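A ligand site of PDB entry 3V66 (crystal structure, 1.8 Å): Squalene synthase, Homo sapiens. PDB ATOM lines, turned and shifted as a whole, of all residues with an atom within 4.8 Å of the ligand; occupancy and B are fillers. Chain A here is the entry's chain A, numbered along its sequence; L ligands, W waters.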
ATOM      1  N   SER A  23      15.376 -22.345   2.714  1.00  0.00           N
ATOM      2  CA  SER A  23      15.783 -23.660   2.206  1.00  0.00           C
ATOM      3  C   SER A  23      16.570 -24.449   3.248  1.00  0.00           C
ATOM      4  O   SER A  23      16.825 -25.636   3.079  1.00  0.00           O
ATOM      5  CB  SER A  23      16.615 -23.529   0.919  1.00  0.00           C
ATOM      6  OG  SER A  23      17.809 -22.810   1.161  1.00  0.00           O
ATOM      7  N   PHE A  24      16.936 -23.801   4.340  1.00  0.00           N
ATOM      8  CA  PHE A  24      17.651 -24.499   5.383  1.00  0.00           C
ATOM      9  C   PHE A  24      16.714 -25.284   6.275  1.00  0.00           C
ATOM     10  O   PHE A  24      17.130 -26.240   6.898  1.00  0.00           O
ATOM     11  CB  PHE A  24      18.535 -23.564   6.192  1.00  0.00           C
ATOM     12  CG  PHE A  24      19.645 -24.276   6.922  1.00  0.00           C
ATOM     13  CD1 PHE A  24      20.379 -25.268   6.288  1.00  0.00           C
ATOM     14  CD2 PHE A  24      19.941 -23.944   8.229  1.00  0.00           C
ATOM     15  CE1 PHE A  24      21.417 -25.939   6.949  1.00  0.00           C
ATOM     16  CE2 PHE A  24      20.984 -24.598   8.904  1.00  0.00           C
ATOM     17  CZ  PHE A  24      21.715 -25.600   8.268  1.00  0.00           C
ATOM     18  N   VAL A  39      16.414 -29.015  17.618  1.00  0.00           N
ATOM     19  CA  VAL A  39      17.119 -28.039  16.775  1.00  0.00           C
ATOM     20  C   VAL A  39      16.159 -26.985  16.195  1.00  0.00           C
ATOM     21  O   VAL A  39      16.526 -25.806  16.078  1.00  0.00           O
ATOM     22  CB  VAL A  39      17.891 -28.740  15.655  1.00  0.00           C
ATOM     23  CG1 VAL A  39      18.493 -27.692  14.665  1.00  0.00           C
ATOM     24  CG2 VAL A  39      18.981 -29.637  16.230  1.00  0.00           C
ATOM     25  N   PHE A  42      15.675 -24.651  19.092  1.00  0.00           N
ATOM     26  CA  PHE A  42      16.911 -23.883  19.356  1.00  0.00           C
ATOM     27  C   PHE A  42      17.105 -22.826  18.270  1.00  0.00           C
ATOM     28  O   PHE A  42      17.492 -21.697  18.562  1.00  0.00           O
ATOM     29  CB  PHE A  42      18.126 -24.827  19.360  1.00  0.00           C
ATOM     30  CG  PHE A  42      19.401 -24.215  19.904  1.00  0.00           C
ATOM     31  CD1 PHE A  42      20.640 -24.747  19.524  1.00  0.00           C
ATOM     32  CD2 PHE A  42      19.377 -23.194  20.833  1.00  0.00           C
ATOM     33  CE1 PHE A  42      21.855 -24.219  20.029  1.00  0.00           C
ATOM     34  CE2 PHE A  42      20.575 -22.647  21.370  1.00  0.00           C
ATOM     35  CZ  PHE A  42      21.799 -23.155  20.994  1.00  0.00           C
ATOM     36  N   TYR A  43      16.871 -23.193  17.022  1.00  0.00           N
ATOM     37  CA  TYR A  43      17.040 -22.242  15.927  1.00  0.00           C
ATOM     38  C   TYR A  43      16.134 -21.018  16.153  1.00  0.00           C
ATOM     39  O   TYR A  43      16.581 -19.893  16.001  1.00  0.00           O
ATOM     40  CB  TYR A  43      16.689 -22.888  14.582  1.00  0.00           C
ATOM     41  CG  TYR A  43      16.978 -21.961  13.409  1.00  0.00           C
ATOM     42  CD1 TYR A  43      18.180 -22.030  12.721  1.00  0.00           C
ATOM     43  CD2 TYR A  43      16.032 -21.006  13.006  1.00  0.00           C
ATOM     44  CE1 TYR A  43      18.430 -21.171  11.625  1.00  0.00           C
ATOM     45  CE2 TYR A  43      16.284 -20.140  11.922  1.00  0.00           C
ATOM     46  CZ  TYR A  43      17.480 -20.230  11.250  1.00  0.00           C
ATOM     47  OH  TYR A  43      17.725 -19.393  10.160  1.00  0.00           O
ATOM     48  N   LEU A  46      17.218 -18.821  19.157  1.00  0.00           N
ATOM     49  CA  LEU A  46      18.384 -18.030  18.718  1.00  0.00           C
ATOM     50  C   LEU A  46      17.961 -16.871  17.804  1.00  0.00           C
ATOM     51  O   LEU A  46      18.490 -15.767  17.887  1.00  0.00           O
ATOM     52  CB  LEU A  46      19.368 -18.928  17.994  1.00  0.00           C
ATOM     53  CG  LEU A  46      20.101 -19.907  18.948  1.00  0.00           C
ATOM     54  CD1 LEU A  46      20.846 -20.999  18.114  1.00  0.00           C
ATOM     55  CD2 LEU A  46      21.099 -19.171  19.842  1.00  0.00           C
ATOM     56  N   ALA A 146      28.114 -17.043  17.618  1.00  0.00           N
ATOM     57  CA  ALA A 146      28.112 -18.212  16.733  1.00  0.00           C
ATOM     58  C   ALA A 146      28.844 -19.447  17.277  1.00  0.00           C
ATOM     59  O   ALA A 146      28.353 -20.569  17.132  1.00  0.00           O
ATOM     60  CB  ALA A 146      28.664 -17.838  15.338  1.00  0.00           C
ATOM     61  N   VAL A 149      26.705 -21.262  19.530  1.00  0.00           N
ATOM     62  CA  VAL A 149      25.671 -22.047  18.779  1.00  0.00           C
ATOM     63  C   VAL A 149      26.215 -23.425  18.381  1.00  0.00           C
ATOM     64  O   VAL A 149      25.531 -24.465  18.543  1.00  0.00           O
ATOM     65  CB  VAL A 149      25.176 -21.310  17.482  1.00  0.00           C
ATOM     66  CG1 VAL A 149      24.133 -22.176  16.726  1.00  0.00           C
ATOM     67  CG2 VAL A 149      24.607 -19.959  17.833  1.00  0.00           C
ATOM     68  N   GLY A 150      27.429 -23.430  17.837  1.00  0.00           N
ATOM     69  CA  GLY A 150      28.126 -24.677  17.492  1.00  0.00           C
ATOM     70  C   GLY A 150      28.208 -25.601  18.689  1.00  0.00           C
ATOM     71  O   GLY A 150      27.847 -26.781  18.583  1.00  0.00           O
ATOM     72  N   LEU A 153      24.573 -26.950  19.728  1.00  0.00           N
ATOM     73  CA  LEU A 153      24.087 -27.949  18.821  1.00  0.00           C
ATOM     74  C   LEU A 153      24.809 -29.253  19.078  1.00  0.00           C
ATOM     75  O   LEU A 153      24.155 -30.311  19.076  1.00  0.00           O
ATOM     76  CB  LEU A 153      24.258 -27.455  17.372  1.00  0.00           C
ATOM     77  CG  LEU A 153      23.228 -26.381  16.944  1.00  0.00           C
ATOM     78  CD1 LEU A 153      23.717 -25.742  15.663  1.00  0.00           C
ATOM     79  CD2 LEU A 153      21.804 -26.942  16.705  1.00  0.00           C
ATOM     80  N   SER A 154      26.117 -29.179  19.327  1.00  0.00           N
ATOM     81  CA  SER A 154      26.928 -30.372  19.497  1.00  0.00           C
ATOM     82  C   SER A 154      26.445 -31.118  20.729  1.00  0.00           C
ATOM     83  O   SER A 154      26.331 -32.375  20.727  1.00  0.00           O
ATOM     84  CB  SER A 154      28.399 -30.009  19.674  1.00  0.00           C
ATOM     85  OG  SER A 154      28.893 -29.388  18.481  1.00  0.00           O
ATOM     86  N   PHE A 157      23.385 -33.029  19.938  1.00  0.00           N
ATOM     87  CA  PHE A 157      23.713 -34.263  19.205  1.00  0.00           C
ATOM     88  C   PHE A 157      24.131 -35.398  20.163  1.00  0.00           C
ATOM     89  O   PHE A 157      23.646 -36.536  20.046  1.00  0.00           O
ATOM     90  CB  PHE A 157      24.844 -34.061  18.173  1.00  0.00           C
ATOM     91  CG  PHE A 157      24.595 -32.956  17.160  1.00  0.00           C
ATOM     92  CD1 PHE A 157      25.697 -32.267  16.627  1.00  0.00           C
ATOM     93  CD2 PHE A 157      23.310 -32.607  16.742  1.00  0.00           C
ATOM     94  CE1 PHE A 157      25.521 -31.236  15.697  1.00  0.00           C
ATOM     95  CE2 PHE A 157      23.125 -31.576  15.770  1.00  0.00           C
ATOM     96  CZ  PHE A 157      24.238 -30.878  15.281  1.00  0.00           C
ATOM     97  N   MET A 177      33.509 -24.399  14.263  1.00  0.00           N
ATOM     98  CA  MET A 177      32.375 -24.499  13.319  1.00  0.00           C
ATOM     99  C   MET A 177      31.612 -23.182  13.214  1.00  0.00           C
ATOM    100  O   MET A 177      31.377 -22.672  12.129  1.00  0.00           O
ATOM    101  CB  MET A 177      31.440 -25.667  13.697  1.00  0.00           C
ATOM    102  CG  MET A 177      32.095 -27.062  13.638  1.00  0.00           C
ATOM    103  SD  MET A 177      32.189 -27.649  11.925  1.00  0.00           S
ATOM    104  CE  MET A 177      30.467 -27.965  11.537  1.00  0.00           C
ATOM    105  N   GLY A 178      31.260 -22.608  14.370  1.00  0.00           N
ATOM    106  CA  GLY A 178      30.671 -21.279  14.421  1.00  0.00           C
ATOM    107  C   GLY A 178      31.525 -20.115  13.945  1.00  0.00           C
ATOM    108  O   GLY A 178      31.004 -19.264  13.236  1.00  0.00           O
ATOM    109  N   LEU A 181      31.827 -19.901  10.056  1.00  0.00           N
ATOM    110  CA  LEU A 181      30.635 -19.356   9.424  1.00  0.00           C
ATOM    111  C   LEU A 181      30.500 -17.871   9.693  1.00  0.00           C
ATOM    112  O   LEU A 181      30.243 -17.094   8.775  1.00  0.00           O
ATOM    113  CB  LEU A 181      29.360 -20.084   9.887  1.00  0.00           C
ATOM    114  CG  LEU A 181      29.375 -21.598   9.645  1.00  0.00           C
ATOM    115  CD1 LEU A 181      28.101 -22.273  10.209  1.00  0.00           C
ATOM    116  CD2 LEU A 181      29.480 -21.901   8.135  1.00  0.00           C
ATOM    117  N   GLN A 182      30.668 -17.480  10.952  1.00  0.00           N
ATOM    118  CA  GLN A 182      30.469 -16.080  11.305  1.00  0.00           C
ATOM    119  C   GLN A 182      31.470 -15.140  10.617  1.00  0.00           C
ATOM    120  O   GLN A 182      31.102 -14.055  10.141  1.00  0.00           O
ATOM    121  CB  GLN A 182      30.525 -15.921  12.831  1.00  0.00           C
ATOM    122  CG  GLN A 182      29.993 -14.531  13.262  1.00  0.00           C
ATOM    123  CD  GLN A 182      28.525 -14.374  12.982  1.00  0.00           C
ATOM    124  OE1 GLN A 182      27.767 -15.359  12.946  1.00  0.00           O
ATOM    125  NE2 GLN A 182      28.106 -13.136  12.754  1.00  0.00           N
ATOM    126  N   ASN A 185      30.603 -14.717   6.963  1.00  0.00           N
ATOM    127  CA  ASN A 185      29.523 -13.739   6.831  1.00  0.00           C
ATOM    128  C   ASN A 185      30.037 -12.297   7.073  1.00  0.00           C
ATOM    129  O   ASN A 185      29.767 -11.388   6.299  1.00  0.00           O
ATOM    130  CB  ASN A 185      28.378 -14.098   7.773  1.00  0.00           C
ATOM    131  CG  ASN A 185      27.553 -15.278   7.251  1.00  0.00           C
ATOM    132  OD1 ASN A 185      27.582 -15.569   6.043  1.00  0.00           O
ATOM    133  ND2 ASN A 185      26.803 -15.926   8.128  1.00  0.00           N
ATOM    134  N   TYR A 246      35.950 -31.893  13.197  1.00  0.00           N
ATOM    135  CA  TYR A 246      34.577 -31.958  13.698  1.00  0.00           C
ATOM    136  C   TYR A 246      33.675 -32.845  12.825  1.00  0.00           C
ATOM    137  O   TYR A 246      33.007 -33.791  13.300  1.00  0.00           O
ATOM    138  CB  TYR A 246      34.005 -30.549  13.805  1.00  0.00           C
ATOM    139  CG  TYR A 246      32.598 -30.530  14.400  1.00  0.00           C
ATOM    140  CD1 TYR A 246      31.497 -30.780  13.605  1.00  0.00           C
ATOM    141  CD2 TYR A 246      32.409 -30.289  15.792  1.00  0.00           C
ATOM    142  CE1 TYR A 246      30.184 -30.760  14.135  1.00  0.00           C
ATOM    143  CE2 TYR A 246      31.114 -30.233  16.330  1.00  0.00           C
ATOM    144  CZ  TYR A 246      30.032 -30.494  15.514  1.00  0.00           C
ATOM    145  OH  TYR A 246      28.772 -30.467  16.048  1.00  0.00           O
ATOM    146  N   PHE A 258      23.431 -31.789   8.054  1.00  0.00           N
ATOM    147  CA  PHE A 258      23.115 -30.507   8.735  1.00  0.00           C
ATOM    148  C   PHE A 258      24.379 -29.709   9.025  1.00  0.00           C
ATOM    149  O   PHE A 258      24.401 -28.473   8.814  1.00  0.00           O
ATOM    150  CB  PHE A 258      22.367 -30.807  10.038  1.00  0.00           C
ATOM    151  CG  PHE A 258      22.094 -29.584  10.925  1.00  0.00           C
ATOM    152  CD1 PHE A 258      22.597 -29.550  12.224  1.00  0.00           C
ATOM    153  CD2 PHE A 258      21.318 -28.525  10.480  1.00  0.00           C
ATOM    154  CE1 PHE A 258      22.338 -28.447  13.060  1.00  0.00           C
ATOM    155  CE2 PHE A 258      21.062 -27.409  11.308  1.00  0.00           C
ATOM    156  CZ  PHE A 258      21.564 -27.382  12.586  1.00  0.00           C
ATOM    157  N   CYS A 259      25.427 -30.401   9.511  1.00  0.00           N
ATOM    158  CA  CYS A 259      26.670 -29.725   9.860  1.00  0.00           C
ATOM    159  C   CYS A 259      27.527 -29.303   8.666  1.00  0.00           C
ATOM    160  O   CYS A 259      28.164 -28.231   8.669  1.00  0.00           O
ATOM    161  CB  CYS A 259      27.504 -30.585  10.781  1.00  0.00           C
ATOM    162  SG  CYS A 259      26.741 -30.739  12.434  1.00  0.00           S
ATOM    163  N   ILE A 261      26.647 -28.866   5.340  1.00  0.00           N
ATOM    164  CA  ILE A 261      26.064 -27.909   4.371  1.00  0.00           C
ATOM    165  C   ILE A 261      26.560 -26.460   4.542  1.00  0.00           C
ATOM    166  O   ILE A 261      27.093 -25.869   3.570  1.00  0.00           O
ATOM    167  CB  ILE A 261      24.510 -28.051   4.287  1.00  0.00           C
ATOM    168  CG1 ILE A 261      24.172 -29.325   3.485  1.00  0.00           C
ATOM    169  CG2 ILE A 261      23.872 -26.820   3.647  1.00  0.00           C
ATOM    170  CD1 ILE A 261      22.659 -29.756   3.558  1.00  0.00           C
ATOM    171  N   PRO A 262      26.456 -25.879   5.745  1.00  0.00           N
ATOM    172  CA  PRO A 262      26.946 -24.500   5.904  1.00  0.00           C
ATOM    173  C   PRO A 262      28.438 -24.386   5.663  1.00  0.00           C
ATOM    174  O   PRO A 262      28.911 -23.358   5.160  1.00  0.00           O
ATOM    175  CB  PRO A 262      26.627 -24.190   7.372  1.00  0.00           C
ATOM    176  CG  PRO A 262      25.381 -25.076   7.637  1.00  0.00           C
ATOM    177  CD  PRO A 262      25.849 -26.364   7.016  1.00  0.00           C
ATOM    178  N   MET A 265      29.292 -24.301   1.939  1.00  0.00           N
ATOM    179  CA  MET A 265      28.855 -23.040   1.388  1.00  0.00           C
ATOM    180  C   MET A 265      29.715 -21.851   1.822  1.00  0.00           C
ATOM    181  O   MET A 265      29.969 -20.951   0.998  1.00  0.00           O
ATOM    182  CB  MET A 265      27.362 -22.810   1.638  1.00  0.00           C
ATOM    183  CG  MET A 265      26.484 -23.803   0.850  1.00  0.00           C
ATOM    184  SD  MET A 265      24.782 -23.693   1.330  1.00  0.00           S
ATOM    185  CE  MET A 265      24.330 -22.075   0.677  1.00  0.00           C
ATOM    186  N   MET A 295      25.138 -28.514  -1.621  1.00  0.00           N
ATOM    187  CA  MET A 295      24.272 -29.118  -0.612  1.00  0.00           C
ATOM    188  C   MET A 295      24.026 -30.604  -0.896  1.00  0.00           C
ATOM    189  O   MET A 295      24.134 -31.446   0.002  1.00  0.00           O
ATOM    190  CB  MET A 295      22.954 -28.337  -0.509  1.00  0.00           C
ATOM    191  CG  MET A 295      23.176 -26.926   0.035  1.00  0.00           C
ATOM    192  SD  MET A 295      21.693 -26.027   0.544  1.00  0.00           S
ATOM    193  CE  MET A 295      20.881 -25.698  -1.016  1.00  0.00           C
HETATM  194  C1  LIG L   1      27.861 -23.350  14.054  1.00  0.00           C
HETATM  195  O1  LIG L   1      26.458 -23.705  14.137  1.00  0.00           O
HETATM  196  C2  LIG L   1      25.981 -24.703  13.323  1.00  0.00           C
HETATM  197  C3  LIG L   1      26.332 -26.061  13.496  1.00  0.00           C
HETATM  198  O2  LIG L   1      27.179 -26.335  14.560  1.00  0.00           O
HETATM  199  C4  LIG L   1      27.560 -27.679  14.900  1.00  0.00           C
HETATM  200  C5  LIG L   1      25.767 -27.042  12.649  1.00  0.00           C
HETATM  201  C6  LIG L   1      24.908 -26.688  11.618  1.00  0.00           C
HETATM  202  C7  LIG L   1      24.574 -25.345  11.444  1.00  0.00           C
HETATM  203  C8  LIG L   1      25.118 -24.368  12.289  1.00  0.00           C
HETATM  204  C9  LIG L   1      24.733 -22.903  12.031  1.00  0.00           C
HETATM  205  C10 LIG L   1      23.561 -22.352  12.835  1.00  0.00           C
HETATM  206  O3  LIG L   1      24.475 -22.648  10.615  1.00  0.00           O
HETATM  207  C11 LIG L   1      24.037 -21.336  10.184  1.00  0.00           C
HETATM  208  C12 LIG L   1      24.655 -20.216  11.059  1.00  0.00           C
HETATM  209  C13 LIG L   1      25.614 -19.244  10.750  1.00  0.00           C
HETATM  210  C14 LIG L   1      25.843 -18.522  11.897  1.00  0.00           C
HETATM  211  C15 LIG L   1      25.038 -19.039  12.925  1.00  0.00           C
HETATM  212  N1  LIG L   1      24.310 -20.111  12.428  1.00  0.00           N
HETATM  213  C16 LIG L   1      23.412 -20.935  12.980  1.00  0.00           C
HETATM  214  C17 LIG L   1      22.309 -20.489  13.761  1.00  0.00           C
HETATM  215  C18 LIG L   1      21.431 -21.400  14.309  1.00  0.00           C
HETATM  216  C19 LIG L   1      21.592 -22.766  14.153  1.00  0.00           C
HETATM  217  C20 LIG L   1      22.640 -23.270  13.420  1.00  0.00           C
HETATM  218 CL1  LIG L   1      20.432 -23.852  14.877  1.00  0.00          CL
HETATM  219  C21 LIG L   1      24.244 -21.386   8.643  1.00  0.00           C
HETATM  220  C22 LIG L   1      23.084 -20.720   7.881  1.00  0.00           C
HETATM  221  O4  LIG L   1      22.161 -20.213   8.551  1.00  0.00           O
HETATM  222  N2  LIG L   1      23.081 -20.684   6.535  1.00  0.00           N
HETATM  223  C23 LIG L   1      21.833 -20.253   5.798  1.00  0.00           C
HETATM  224  C24 LIG L   1      21.265 -21.380   4.895  1.00  0.00           C
HETATM  225  C25 LIG L   1      22.331 -22.241   4.152  1.00  0.00           C
HETATM  226  C26 LIG L   1      23.542 -22.640   5.034  1.00  0.00           C
HETATM  227  C27 LIG L   1      24.146 -21.423   5.752  1.00  0.00           C
HETATM  228  C28 LIG L   1      21.697 -23.492   3.487  1.00  0.00           C
HETATM  229  C29 LIG L   1      20.642 -23.184   2.446  1.00  0.00           C
HETATM  230  O5  LIG L   1      20.886 -22.282   1.622  1.00  0.00           O
HETATM  231  O6  LIG L   1      19.579 -23.845   2.457  1.00  0.00           O
HETATM  232  O   HOH W   1      27.966 -25.990  10.154  1.00  0.00           O
HETATM  233  O   HOH W   2      27.292 -21.066   4.988  1.00  0.00           O
HETATM  234  O   HOH W   3      22.247 -17.833  10.832  1.00  0.00           O
HETATM  235  O   HOH W   4      26.714 -19.635   7.030  1.00  0.00           O
HETATM  236  O   HOH W   5      18.890 -19.107  14.444  1.00  0.00           O
HETATM  237  O   HOH W   6      22.480 -17.618   8.189  1.00  0.00           O
HETATM  238  O   HOH W   7      21.911 -17.517  15.442  1.00  0.00           O
HETATM  239  O   HOH W   8      19.487 -20.325   8.321  1.00  0.00           O
HETATM  240  O   HOH W   9      20.528 -26.077   2.923  1.00  0.00           O
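The side-chain hydroxyl (OG) of Ser 23 sits at hydrogen-bond distance from an oxygen (O6) of the ligand, 2.4 Å away. O6 of the ligand sits at hydrogen-bond distance from N of Phe 24.
The side-chain hydroxyl (OH) of Tyr 246 sits at hydrogen-bond distance from the side-chain hydroxyl (OG) of Ser 154, 2.7 Å away. The side-chain hydroxyl (OG) of Ser 154 is in hydrogen-bond range of the backbone carbonyl oxygen (O) of Gly 150 (2.8 Å).
The side-chain sulfur (SD) of Met 295 lies close to an oxygen (O6) of the ligand. Merely in contact with the ligand: Tyr 246 (3.2 Å), Phe 258 (3.4 Å), Leu 153 (3.4 Å), Gly 178 (3.5 Å), Gly 150 (3.5 Å), Met 265 (3.6 Å), Tyr 43 (3.6 Å), Val 149 (3.7 Å), Leu 181 (3.7 Å), Cys 259 (3.8 Å), Met 177 (3.8 Å), Gln 182 (3.8 Å), Leu 46 (3.9 Å), Pro 262 (3.9 Å) and Ile 261 (3.98 Å). Hydrophobic or aromatic side chains that line the ligand: Phe 24, Tyr 43, Leu 46, Val 149, Leu 153, Leu 181, Tyr 246, Phe 258, Ile 261, Pro 262, Met 265 and Met 295. 18 residues have an atom within 4 Å of the ligand: Ser 23, Phe 24, Tyr 43, Leu 46, Val 149, Gly 150, Leu 153, Met 177, Gly 178, Leu 181, Gln 182, Tyr 246, Phe 258, Cys 259, Ile 261, Pro 262, Met 265 and Met 295. The nearest printed residue that does not touch the ligand is Phe 157 (4.2 Å).
Water W9 lies within hydrogen-bond range of an oxygen (O6) of the ligand (2.5 Å) and the side-chain sulfur (SD) of Met 295 (2.6 Å). Water W8 lies within hydrogen-bond range of an oxygen (O4) of the ligand and the side-chain hydroxyl (OH) of Tyr 43.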
